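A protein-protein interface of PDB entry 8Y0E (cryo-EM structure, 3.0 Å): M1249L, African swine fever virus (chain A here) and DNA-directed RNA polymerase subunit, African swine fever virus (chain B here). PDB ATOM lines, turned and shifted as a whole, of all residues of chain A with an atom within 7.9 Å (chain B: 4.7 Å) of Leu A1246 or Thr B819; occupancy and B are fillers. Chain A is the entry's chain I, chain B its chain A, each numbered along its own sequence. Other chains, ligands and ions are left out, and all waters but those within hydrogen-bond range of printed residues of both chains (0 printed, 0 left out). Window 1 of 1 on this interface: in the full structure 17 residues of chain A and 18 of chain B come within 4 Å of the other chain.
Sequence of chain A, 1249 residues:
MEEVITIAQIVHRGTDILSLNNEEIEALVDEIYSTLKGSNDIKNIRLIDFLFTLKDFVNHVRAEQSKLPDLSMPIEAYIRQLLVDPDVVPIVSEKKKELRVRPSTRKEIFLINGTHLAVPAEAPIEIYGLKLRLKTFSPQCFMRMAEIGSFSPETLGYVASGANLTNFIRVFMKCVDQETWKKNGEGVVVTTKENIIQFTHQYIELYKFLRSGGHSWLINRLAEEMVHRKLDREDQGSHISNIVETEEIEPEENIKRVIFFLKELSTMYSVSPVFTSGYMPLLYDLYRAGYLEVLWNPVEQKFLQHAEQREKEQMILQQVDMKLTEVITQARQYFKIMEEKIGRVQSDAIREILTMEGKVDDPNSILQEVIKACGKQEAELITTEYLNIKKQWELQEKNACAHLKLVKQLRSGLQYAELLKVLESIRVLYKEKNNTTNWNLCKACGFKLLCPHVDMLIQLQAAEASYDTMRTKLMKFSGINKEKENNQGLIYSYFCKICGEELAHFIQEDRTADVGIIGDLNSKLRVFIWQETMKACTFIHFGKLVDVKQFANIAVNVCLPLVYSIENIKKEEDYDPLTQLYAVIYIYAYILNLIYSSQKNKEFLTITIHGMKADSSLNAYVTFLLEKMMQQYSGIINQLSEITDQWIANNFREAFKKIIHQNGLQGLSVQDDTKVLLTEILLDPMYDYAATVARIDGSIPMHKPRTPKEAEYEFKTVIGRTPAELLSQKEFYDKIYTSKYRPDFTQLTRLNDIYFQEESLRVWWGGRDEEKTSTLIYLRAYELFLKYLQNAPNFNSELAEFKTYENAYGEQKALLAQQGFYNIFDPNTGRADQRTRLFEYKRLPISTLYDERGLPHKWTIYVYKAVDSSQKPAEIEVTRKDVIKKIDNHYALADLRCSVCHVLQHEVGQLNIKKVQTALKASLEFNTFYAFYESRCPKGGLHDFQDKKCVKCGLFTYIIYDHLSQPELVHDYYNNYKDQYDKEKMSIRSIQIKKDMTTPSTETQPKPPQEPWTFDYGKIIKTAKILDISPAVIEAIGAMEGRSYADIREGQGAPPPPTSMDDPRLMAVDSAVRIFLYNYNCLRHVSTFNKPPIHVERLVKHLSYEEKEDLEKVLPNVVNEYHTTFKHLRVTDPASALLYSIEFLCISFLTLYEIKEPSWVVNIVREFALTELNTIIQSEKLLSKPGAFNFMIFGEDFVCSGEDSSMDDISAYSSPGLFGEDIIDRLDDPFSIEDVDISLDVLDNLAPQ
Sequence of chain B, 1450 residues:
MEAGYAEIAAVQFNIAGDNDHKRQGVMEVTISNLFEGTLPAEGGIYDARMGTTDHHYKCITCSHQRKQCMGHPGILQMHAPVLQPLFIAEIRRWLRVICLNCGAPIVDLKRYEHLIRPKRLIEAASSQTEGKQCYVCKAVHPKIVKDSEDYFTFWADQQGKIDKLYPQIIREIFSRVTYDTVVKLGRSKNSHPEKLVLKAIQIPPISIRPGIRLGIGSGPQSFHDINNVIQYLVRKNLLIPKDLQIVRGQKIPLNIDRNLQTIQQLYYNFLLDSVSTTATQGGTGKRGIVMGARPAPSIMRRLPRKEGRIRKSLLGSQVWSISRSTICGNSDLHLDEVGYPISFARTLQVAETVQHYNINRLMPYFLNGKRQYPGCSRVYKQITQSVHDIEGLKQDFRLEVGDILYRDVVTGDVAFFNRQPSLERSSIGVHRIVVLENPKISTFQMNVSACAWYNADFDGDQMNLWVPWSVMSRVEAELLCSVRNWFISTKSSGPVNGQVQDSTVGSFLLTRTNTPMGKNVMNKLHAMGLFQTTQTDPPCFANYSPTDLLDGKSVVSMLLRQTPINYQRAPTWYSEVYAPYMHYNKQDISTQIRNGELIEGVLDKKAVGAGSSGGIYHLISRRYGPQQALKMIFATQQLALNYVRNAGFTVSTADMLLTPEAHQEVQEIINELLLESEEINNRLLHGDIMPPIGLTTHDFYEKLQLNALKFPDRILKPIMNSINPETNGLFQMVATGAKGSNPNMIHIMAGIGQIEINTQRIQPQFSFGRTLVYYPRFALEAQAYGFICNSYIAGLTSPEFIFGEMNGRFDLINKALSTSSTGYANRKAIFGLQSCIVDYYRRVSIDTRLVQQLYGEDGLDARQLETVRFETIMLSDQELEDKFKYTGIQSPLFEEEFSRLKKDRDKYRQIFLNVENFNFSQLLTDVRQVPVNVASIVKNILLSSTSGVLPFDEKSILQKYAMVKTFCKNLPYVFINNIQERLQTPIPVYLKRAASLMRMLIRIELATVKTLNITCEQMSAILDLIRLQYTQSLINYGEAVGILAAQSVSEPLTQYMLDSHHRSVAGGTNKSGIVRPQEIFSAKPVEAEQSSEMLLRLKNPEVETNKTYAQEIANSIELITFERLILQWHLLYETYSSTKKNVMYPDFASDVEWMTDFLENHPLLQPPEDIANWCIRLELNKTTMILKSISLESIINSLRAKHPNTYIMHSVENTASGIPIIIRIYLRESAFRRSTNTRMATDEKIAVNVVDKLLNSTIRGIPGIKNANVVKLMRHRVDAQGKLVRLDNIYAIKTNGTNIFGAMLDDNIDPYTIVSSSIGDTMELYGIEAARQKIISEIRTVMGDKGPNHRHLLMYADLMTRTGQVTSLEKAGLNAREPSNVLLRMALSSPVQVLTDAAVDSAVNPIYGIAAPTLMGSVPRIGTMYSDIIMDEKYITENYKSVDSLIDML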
ATOM      1  N   PRO A1230       8.431  -5.137   9.175  1.00  0.00           N
ATOM      2  CA  PRO A1230       9.450  -6.102   9.608  1.00  0.00           C
ATOM      3  C   PRO A1230      10.092  -6.823   8.437  1.00  0.00           C
ATOM      4  O   PRO A1230      10.407  -8.010   8.528  1.00  0.00           O
ATOM      5  CB  PRO A1230       8.664  -7.078  10.498  1.00  0.00           C
ATOM      6  CG  PRO A1230       7.203  -6.697  10.369  1.00  0.00           C
ATOM      7  CD  PRO A1230       7.074  -5.696   9.269  1.00  0.00           C
ATOM      8  N   PHE A1231      10.315  -6.108   7.347  1.00  0.00           N
ATOM      9  CA  PHE A1231      11.000  -6.686   6.200  1.00  0.00           C
ATOM     10  C   PHE A1231      11.969  -5.722   5.539  1.00  0.00           C
ATOM     11  O   PHE A1231      12.550  -6.078   4.511  1.00  0.00           O
ATOM     12  CB  PHE A1231       9.977  -7.174   5.165  1.00  0.00           C
ATOM     13  CG  PHE A1231       9.780  -8.658   5.163  1.00  0.00           C
ATOM     14  CD1 PHE A1231      10.801  -9.503   4.777  1.00  0.00           C
ATOM     15  CD2 PHE A1231       8.570  -9.207   5.534  1.00  0.00           C
ATOM     16  CE1 PHE A1231      10.619 -10.866   4.772  1.00  0.00           C
ATOM     17  CE2 PHE A1231       8.382 -10.571   5.524  1.00  0.00           C
ATOM     18  CZ  PHE A1231       9.411 -11.401   5.146  1.00  0.00           C
ATOM     19  N   SER A1232      12.165  -4.527   6.080  1.00  0.00           N
ATOM     20  CA  SER A1232      12.913  -3.476   5.413  1.00  0.00           C
ATOM     21  C   SER A1232      14.338  -3.399   5.940  1.00  0.00           C
ATOM     22  O   SER A1232      14.665  -3.909   7.014  1.00  0.00           O
ATOM     23  CB  SER A1232      12.217  -2.124   5.591  1.00  0.00           C
ATOM     24  OG  SER A1232      11.246  -1.915   4.581  1.00  0.00           O
ATOM     25  N   ILE A1233      15.185  -2.744   5.155  1.00  0.00           N
ATOM     26  CA  ILE A1233      16.553  -2.451   5.544  1.00  0.00           C
ATOM     27  C   ILE A1233      16.670  -1.024   6.083  1.00  0.00           C
ATOM     28  O   ILE A1233      17.752  -0.445   6.075  1.00  0.00           O
ATOM     29  CB  ILE A1233      17.528  -2.700   4.382  1.00  0.00           C
ATOM     30  CG1 ILE A1233      17.089  -3.926   3.580  1.00  0.00           C
ATOM     31  CG2 ILE A1233      18.936  -2.949   4.884  1.00  0.00           C
ATOM     32  CD1 ILE A1233      17.143  -5.222   4.372  1.00  0.00           C
ATOM     33  N   ASP A1235      16.543   0.202   9.104  1.00  0.00           N
ATOM     34  CA  ASP A1235      17.429   0.311  10.254  1.00  0.00           C
ATOM     35  C   ASP A1235      18.691  -0.530  10.125  1.00  0.00           C
ATOM     36  O   ASP A1235      19.572  -0.431  10.985  1.00  0.00           O
ATOM     37  CB  ASP A1235      16.685  -0.073  11.535  1.00  0.00           C
ATOM     38  CG  ASP A1235      15.717   1.003  11.986  1.00  0.00           C
ATOM     39  OD1 ASP A1235      15.063   1.616  11.117  1.00  0.00           O
ATOM     40  OD2 ASP A1235      15.606   1.234  13.207  1.00  0.00           O
ATOM     41  N   VAL A1236      18.800  -1.347   9.086  1.00  0.00           N
ATOM     42  CA  VAL A1236      20.040  -2.048   8.791  1.00  0.00           C
ATOM     43  C   VAL A1236      20.817  -1.223   7.773  1.00  0.00           C
ATOM     44  O   VAL A1236      20.252  -0.422   7.024  1.00  0.00           O
ATOM     45  CB  VAL A1236      19.770  -3.479   8.282  1.00  0.00           C
ATOM     46  CG1 VAL A1236      21.020  -4.336   8.390  1.00  0.00           C
ATOM     47  CG2 VAL A1236      18.619  -4.107   9.052  1.00  0.00           C
ATOM     48  N   ASP A1237      22.139  -1.397   7.752  1.00  0.00           N
ATOM     49  CA  ASP A1237      23.026  -0.539   6.964  1.00  0.00           C
ATOM     50  C   ASP A1237      23.875  -1.393   6.024  1.00  0.00           C
ATOM     51  O   ASP A1237      24.930  -1.899   6.412  1.00  0.00           O
ATOM     52  CB  ASP A1237      23.881   0.314   7.890  1.00  0.00           C
ATOM     53  CG  ASP A1237      23.074   0.920   9.019  1.00  0.00           C
ATOM     54  OD1 ASP A1237      22.322   1.883   8.762  1.00  0.00           O
ATOM     55  OD2 ASP A1237      23.172   0.425  10.159  1.00  0.00           O
ATOM     56  N   ILE A1238      23.403  -1.551   4.787  1.00  0.00           N
ATOM     57  CA  ILE A1238      24.127  -2.261   3.739  1.00  0.00           C
ATOM     58  C   ILE A1238      23.941  -1.491   2.435  1.00  0.00           C
ATOM     59  O   ILE A1238      22.913  -0.844   2.219  1.00  0.00           O
ATOM     60  CB  ILE A1238      23.639  -3.721   3.587  1.00  0.00           C
ATOM     61  CG1 ILE A1238      23.659  -4.444   4.932  1.00  0.00           C
ATOM     62  CG2 ILE A1238      24.520  -4.485   2.619  1.00  0.00           C
ATOM     63  CD1 ILE A1238      22.415  -5.254   5.199  1.00  0.00           C
ATOM     64  N   SER A1239      24.946  -1.557   1.566  1.00  0.00           N
ATOM     65  CA  SER A1239      24.917  -0.894   0.270  1.00  0.00           C
ATOM     66  C   SER A1239      24.576  -1.892  -0.833  1.00  0.00           C
ATOM     67  O   SER A1239      24.549  -3.106  -0.623  1.00  0.00           O
ATOM     68  CB  SER A1239      26.258  -0.210  -0.020  1.00  0.00           C
ATOM     69  OG  SER A1239      26.600   0.693   1.016  1.00  0.00           O
ATOM     70  N   ASP A1241      24.848  -4.211  -4.151  1.00  0.00           N
ATOM     71  CA  ASP A1241      25.832  -5.214  -4.559  1.00  0.00           C
ATOM     72  C   ASP A1241      26.551  -5.772  -3.337  1.00  0.00           C
ATOM     73  O   ASP A1241      27.322  -6.730  -3.440  1.00  0.00           O
ATOM     74  CB  ASP A1241      26.830  -4.641  -5.570  1.00  0.00           C
ATOM     75  CG  ASP A1241      26.269  -4.597  -6.979  1.00  0.00           C
ATOM     76  OD1 ASP A1241      25.220  -5.231  -7.222  1.00  0.00           O
ATOM     77  OD2 ASP A1241      26.873  -3.926  -7.842  1.00  0.00           O
ATOM     78  N   VAL A1242      26.281  -5.183  -2.171  1.00  0.00           N
ATOM     79  CA  VAL A1242      26.698  -5.739  -0.891  1.00  0.00           C
ATOM     80  C   VAL A1242      25.533  -6.432  -0.200  1.00  0.00           C
ATOM     81  O   VAL A1242      25.752  -7.213   0.740  1.00  0.00           O
ATOM     82  CB  VAL A1242      27.314  -4.637   0.001  1.00  0.00           C
ATOM     83  CG1 VAL A1242      27.852  -5.191   1.301  1.00  0.00           C
ATOM     84  CG2 VAL A1242      28.418  -3.923  -0.745  1.00  0.00           C
ATOM     85  N   LEU A1243      24.302  -6.199  -0.661  1.00  0.00           N
ATOM     86  CA  LEU A1243      23.153  -6.982  -0.233  1.00  0.00           C
ATOM     87  C   LEU A1243      23.243  -8.436  -0.679  1.00  0.00           C
ATOM     88  O   LEU A1243      22.468  -9.264  -0.190  1.00  0.00           O
ATOM     89  CB  LEU A1243      21.864  -6.358  -0.771  1.00  0.00           C
ATOM     90  CG  LEU A1243      21.319  -5.136  -0.029  1.00  0.00           C
ATOM     91  CD1 LEU A1243      19.991  -4.706  -0.621  1.00  0.00           C
ATOM     92  CD2 LEU A1243      21.171  -5.430   1.451  1.00  0.00           C
ATOM     93  N   ASP A1244      24.153  -8.762  -1.599  1.00  0.00           N
ATOM     94  CA  ASP A1244      24.392 -10.153  -1.962  1.00  0.00           C
ATOM     95  C   ASP A1244      24.963 -10.958  -0.803  1.00  0.00           C
ATOM     96  O   ASP A1244      24.864 -12.187  -0.809  1.00  0.00           O
ATOM     97  CB  ASP A1244      25.336 -10.231  -3.164  1.00  0.00           C
ATOM     98  CG  ASP A1244      25.033 -11.411  -4.073  1.00  0.00           C
ATOM     99  OD1 ASP A1244      24.842 -12.533  -3.557  1.00  0.00           O
ATOM    100  OD2 ASP A1244      24.982 -11.215  -5.306  1.00  0.00           O
ATOM    101  N   ASN A1245      25.562 -10.294   0.187  1.00  0.00           N
ATOM    102  CA  ASN A1245      26.047 -11.008   1.359  1.00  0.00           C
ATOM    103  C   ASN A1245      24.912 -11.502   2.241  1.00  0.00           C
ATOM    104  O   ASN A1245      25.132 -12.383   3.078  1.00  0.00           O
ATOM    105  CB  ASN A1245      26.985 -10.113   2.165  1.00  0.00           C
ATOM    106  CG  ASN A1245      27.918  -9.319   1.288  1.00  0.00           C
ATOM    107  OD1 ASN A1245      28.208  -9.709   0.161  1.00  0.00           O
ATOM    108  ND2 ASN A1245      28.425  -8.217   1.813  1.00  0.00           N
ATOM    109  N   LEU A1246      23.709 -10.962   2.069  1.00  0.00           N
ATOM    110  CA  LEU A1246      22.532 -11.372   2.821  1.00  0.00           C
ATOM    111  C   LEU A1246      21.778 -12.504   2.141  1.00  0.00           C
ATOM    112  O   LEU A1246      20.697 -12.880   2.604  1.00  0.00           O
ATOM    113  CB  LEU A1246      21.601 -10.176   3.036  1.00  0.00           C
ATOM    114  CG  LEU A1246      22.096  -9.079   3.984  1.00  0.00           C
ATOM    115  CD1 LEU A1246      22.722  -9.689   5.230  1.00  0.00           C
ATOM    116  CD2 LEU A1246      23.075  -8.137   3.293  1.00  0.00           C
ATOM    117  N   ALA A1247      22.327 -13.050   1.058  1.00  0.00           N
ATOM    118  CA  ALA A1247      21.764 -14.172   0.319  1.00  0.00           C
ATOM    119  C   ALA A1247      21.662 -15.392   1.228  1.00  0.00           C
ATOM    120  O   ALA A1247      22.209 -15.379   2.337  1.00  0.00           O
ATOM    121  CB  ALA A1247      22.629 -14.470  -0.909  1.00  0.00           C
ATOM    122  N   PRO A1248      20.959 -16.464   0.808  1.00  0.00           N
ATOM    123  CA  PRO A1248      20.884 -17.674   1.641  1.00  0.00           C
ATOM    124  C   PRO A1248      22.245 -18.189   2.085  1.00  0.00           C
ATOM    125  O   PRO A1248      23.274 -17.823   1.505  1.00  0.00           O
ATOM    126  CB  PRO A1248      20.177 -18.690   0.728  1.00  0.00           C
ATOM    127  CG  PRO A1248      20.058 -18.022  -0.620  1.00  0.00           C
ATOM    128  CD  PRO A1248      20.059 -16.563  -0.351  1.00  0.00           C
ATOM    129  N   GLN A1249      22.248 -19.033   3.116  1.00  0.00           N
ATOM    130  CA  GLN A1249      23.465 -19.512   3.771  1.00  0.00           C
ATOM    131  C   GLN A1249      24.194 -18.352   4.443  1.00  0.00           C
ATOM    132  O   GLN A1249      23.672 -17.241   4.525  1.00  0.00           O
ATOM    133  CB  GLN A1249      24.390 -20.225   2.777  1.00  0.00           C
ATOM    134  CG  GLN A1249      25.258 -21.309   3.391  1.00  0.00           C
ATOM    135  CD  GLN A1249      26.629 -21.381   2.752  1.00  0.00           C
ATOM    136  OE1 GLN A1249      26.753 -21.436   1.530  1.00  0.00           O
ATOM    137  NE2 GLN A1249      27.667 -21.382   3.580  1.00  0.00           N
ATOM    138  OXT GLN A1249      25.315 -18.493   4.931  1.00  0.00           O
ATOM    139  N   GLN B 420      29.880  -6.356   5.155  1.00  0.00           N
ATOM    140  CA  GLN B 420      28.671  -5.806   5.729  1.00  0.00           C
ATOM    141  C   GLN B 420      27.536  -6.816   5.639  1.00  0.00           C
ATOM    142  O   GLN B 420      27.454  -7.578   4.674  1.00  0.00           O
ATOM    143  CB  GLN B 420      28.282  -4.515   5.004  1.00  0.00           C
ATOM    144  CG  GLN B 420      29.454  -3.572   4.793  1.00  0.00           C
ATOM    145  CD  GLN B 420      29.035  -2.230   4.242  1.00  0.00           C
ATOM    146  OE1 GLN B 420      28.987  -2.031   3.031  1.00  0.00           O
ATOM    147  NE2 GLN B 420      28.724  -1.299   5.131  1.00  0.00           N
ATOM    148  N   PRO B 421      26.628  -6.862   6.624  1.00  0.00           N
ATOM    149  CA  PRO B 421      26.512  -5.999   7.805  1.00  0.00           C
ATOM    150  C   PRO B 421      27.549  -6.313   8.870  1.00  0.00           C
ATOM    151  O   PRO B 421      27.899  -7.467   9.088  1.00  0.00           O
ATOM    152  CB  PRO B 421      25.093  -6.296   8.292  1.00  0.00           C
ATOM    153  CG  PRO B 421      24.891  -7.724   7.940  1.00  0.00           C
ATOM    154  CD  PRO B 421      25.596  -7.911   6.624  1.00  0.00           C
ATOM    155  N   LYS B 815      14.256 -16.501   7.450  1.00  0.00           N
ATOM    156  CA  LYS B 815      15.595 -15.980   7.196  1.00  0.00           C
ATOM    157  C   LYS B 815      15.543 -14.526   6.747  1.00  0.00           C
ATOM    158  O   LYS B 815      16.386 -13.716   7.145  1.00  0.00           O
ATOM    159  CB  LYS B 815      16.308 -16.838   6.155  1.00  0.00           C
ATOM    160  CG  LYS B 815      17.823 -16.833   6.270  1.00  0.00           C
ATOM    161  CD  LYS B 815      18.434 -15.659   5.521  1.00  0.00           C
ATOM    162  CE  LYS B 815      17.880 -15.562   4.109  1.00  0.00           C
ATOM    163  NZ  LYS B 815      18.407 -14.380   3.372  1.00  0.00           N
ATOM    164  N   ALA B 816      14.571 -14.178   5.903  1.00  0.00           N
ATOM    165  CA  ALA B 816      14.448 -12.793   5.461  1.00  0.00           C
ATOM    166  C   ALA B 816      14.007 -11.879   6.597  1.00  0.00           C
ATOM    167  O   ALA B 816      14.447 -10.726   6.669  1.00  0.00           O
ATOM    168  CB  ALA B 816      13.477 -12.700   4.287  1.00  0.00           C
ATOM    169  N   LEU B 817      13.135 -12.368   7.482  1.00  0.00           N
ATOM    170  CA  LEU B 817      12.753 -11.608   8.668  1.00  0.00           C
ATOM    171  C   LEU B 817      13.944 -11.366   9.584  1.00  0.00           C
ATOM    172  O   LEU B 817      13.958 -10.387  10.344  1.00  0.00           O
ATOM    173  CB  LEU B 817      11.665 -12.361   9.432  1.00  0.00           C
ATOM    174  CG  LEU B 817      10.236 -12.397   8.900  1.00  0.00           C
ATOM    175  CD1 LEU B 817       9.293 -12.967   9.936  1.00  0.00           C
ATOM    176  CD2 LEU B 817       9.810 -11.012   8.547  1.00  0.00           C
ATOM    177  N   SER B 818      14.920 -12.278   9.556  1.00  0.00           N
ATOM    178  CA  SER B 818      16.042 -12.203  10.486  1.00  0.00           C
ATOM    179  C   SER B 818      16.776 -10.878  10.366  1.00  0.00           C
ATOM    180  O   SER B 818      16.984 -10.182  11.365  1.00  0.00           O
ATOM    181  CB  SER B 818      17.002 -13.364  10.241  1.00  0.00           C
ATOM    182  OG  SER B 818      18.079 -12.958   9.417  1.00  0.00           O
ATOM    183  N   THR B 819      17.172 -10.509   9.148  1.00  0.00           N
ATOM    184  CA  THR B 819      17.961  -9.297   8.969  1.00  0.00           C
ATOM    185  C   THR B 819      17.221  -8.075   9.496  1.00  0.00           C
ATOM    186  O   THR B 819      17.769  -7.307  10.293  1.00  0.00           O
ATOM    187  CB  THR B 819      18.320  -9.114   7.495  1.00  0.00           C
ATOM    188  OG1 THR B 819      19.348 -10.044   7.135  1.00  0.00           O
ATOM    189  CG2 THR B 819      18.809  -7.699   7.233  1.00  0.00           C
ATOM    190  N   SER B 820      15.962  -7.904   9.098  1.00  0.00           N
ATOM    191  CA  SER B 820      15.212  -6.719   9.495  1.00  0.00           C
ATOM    192  C   SER B 820      15.002  -6.659  11.004  1.00  0.00           C
ATOM    193  O   SER B 820      15.307  -5.641  11.640  1.00  0.00           O
ATOM    194  CB  SER B 820      13.868  -6.690   8.769  1.00  0.00           C
ATOM    195  OG  SER B 820      12.875  -7.356   9.526  1.00  0.00           O
ATOM    196  N   SER B 821      14.476  -7.736  11.595  1.00  0.00           N
ATOM    197  CA  SER B 821      14.159  -7.701  13.019  1.00  0.00           C
ATOM    198  C   SER B 821      15.420  -7.556  13.865  1.00  0.00           C
ATOM    199  O   SER B 821      15.450  -6.776  14.829  1.00  0.00           O
ATOM    200  CB  SER B 821      13.386  -8.956  13.412  1.00  0.00           C
ATOM    201  OG  SER B 821      12.922  -8.861  14.743  1.00  0.00           O
ATOM    202  N   THR B 822      16.473  -8.300  13.516  1.00  0.00           N
ATOM    203  CA  THR B 822      17.731  -8.182  14.231  1.00  0.00           C
ATOM    204  C   THR B 822      18.316  -6.788  14.091  1.00  0.00           C
ATOM    205  O   THR B 822      18.863  -6.261  15.058  1.00  0.00           O
ATOM    206  CB  THR B 822      18.715  -9.239  13.728  1.00  0.00           C
ATOM    207  OG1 THR B 822      18.408 -10.501  14.334  1.00  0.00           O
ATOM    208  CG2 THR B 822      20.151  -8.863  14.067  1.00  0.00           C
ATOM    209  N   GLY B 823      18.195  -6.163  12.920  1.00  0.00           N
ATOM    210  CA  GLY B 823      18.698  -4.808  12.772  1.00  0.00           C
ATOM    211  C   GLY B 823      17.959  -3.811  13.642  1.00  0.00           C
ATOM    212  O   GLY B 823      18.577  -2.965  14.290  1.00  0.00           O
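Pro A1230 touches Leu B817 (O to CD2, 3.1 Å).
Phe A1231 touches Ala B816.
Phe A1231 touches Leu B817 (CE2 to CD2, 3.4 Å).
Phe A1231 touches Ser B820.
Ser A1232 touches Ser B820.
Val A1236 touches Thr B819.
Val A1236 touches Gly B823.
Val A1242 touches Gln B420.
Leu A1246 touches Pro B421.
Leu A1246 touches Thr B819 (CD1 to OG1, 3.9 Å).
The backbone carbonyl oxygen of Gln B420 lies within hydrogen-bond range of the side-chain amide nitrogen of Asn A1245 (3.1 Å).
The side-chain amino group (NZ) of Lys B815 sits at hydrogen-bond distance from the backbone carbonyl oxygen (O) of Leu A1246 (2.8 Å).
OG of Ser B820 sits at hydrogen-bond distance from O of Pro A1230 (2.7 Å).
Leu A1246 touches just these residues of chain B: Pro B421, Lys B815 and Thr B819.
Printed residues of chain A within 4 Å of Gln B420: Val A1242 and Asn A1245.
Of the printed residues of chain A, Ala B816 touches Phe A1231.
No residue of chain A comes within 4 Å of Ser B818.
Of chain A, only Val A1236 (3.5 Å) and Leu A1246 (3.9 Å) come within 4 Å of Thr B819.
Of the printed residues of chain A, Ser B820 touches Pro A1230, Phe A1231 and Ser A1232.
The nearest residue of chain A that does not touch Thr B819 is Ile A1233 (4.1 Å).
The nearest printed residue of chain A that does not touch Gly B823 is Asp A1235 (4.3 Å).
Printed residues of chain A that touch a printed residue of chain B: Pro A1230, Phe A1231, Ser A1232, Val A1236, Val A1242, Asn A1245 and Leu A1246.
Hydrophobic or aromatic side chains of chain A that line the printed part of chain B: Phe A1231, Val A1236, Val A1242 and Leu A1246.
Of the 11 printed residues of chain B, 8 touch a printed residue of chain A.
Hydrophobic or aromatic side chains of chain B that line the printed part of chain A: Pro B421, Ala B816 and Leu B817.
Among the printed residues, 13 pairs touch across the chains.
Among the printed residues, no Asp or Glu carboxylate lies within 4 Å of a Lys or Arg side-chain nitrogen of the other chain.
The side-chain hydroxyl (OG) of Ser B818 lies within hydrogen-bond range of the backbone carbonyl oxygen (O) of Lys B815 (2.9 Å).
The backbone carbonyl oxygen of Leu B817 lies within hydrogen-bond range of the side-chain hydroxyl of Ser B820 (3.3 Å).
The backbone carbonyl oxygen of Val A1242 sits at hydrogen-bond distance from the side-chain amide nitrogen of Asn A1245.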
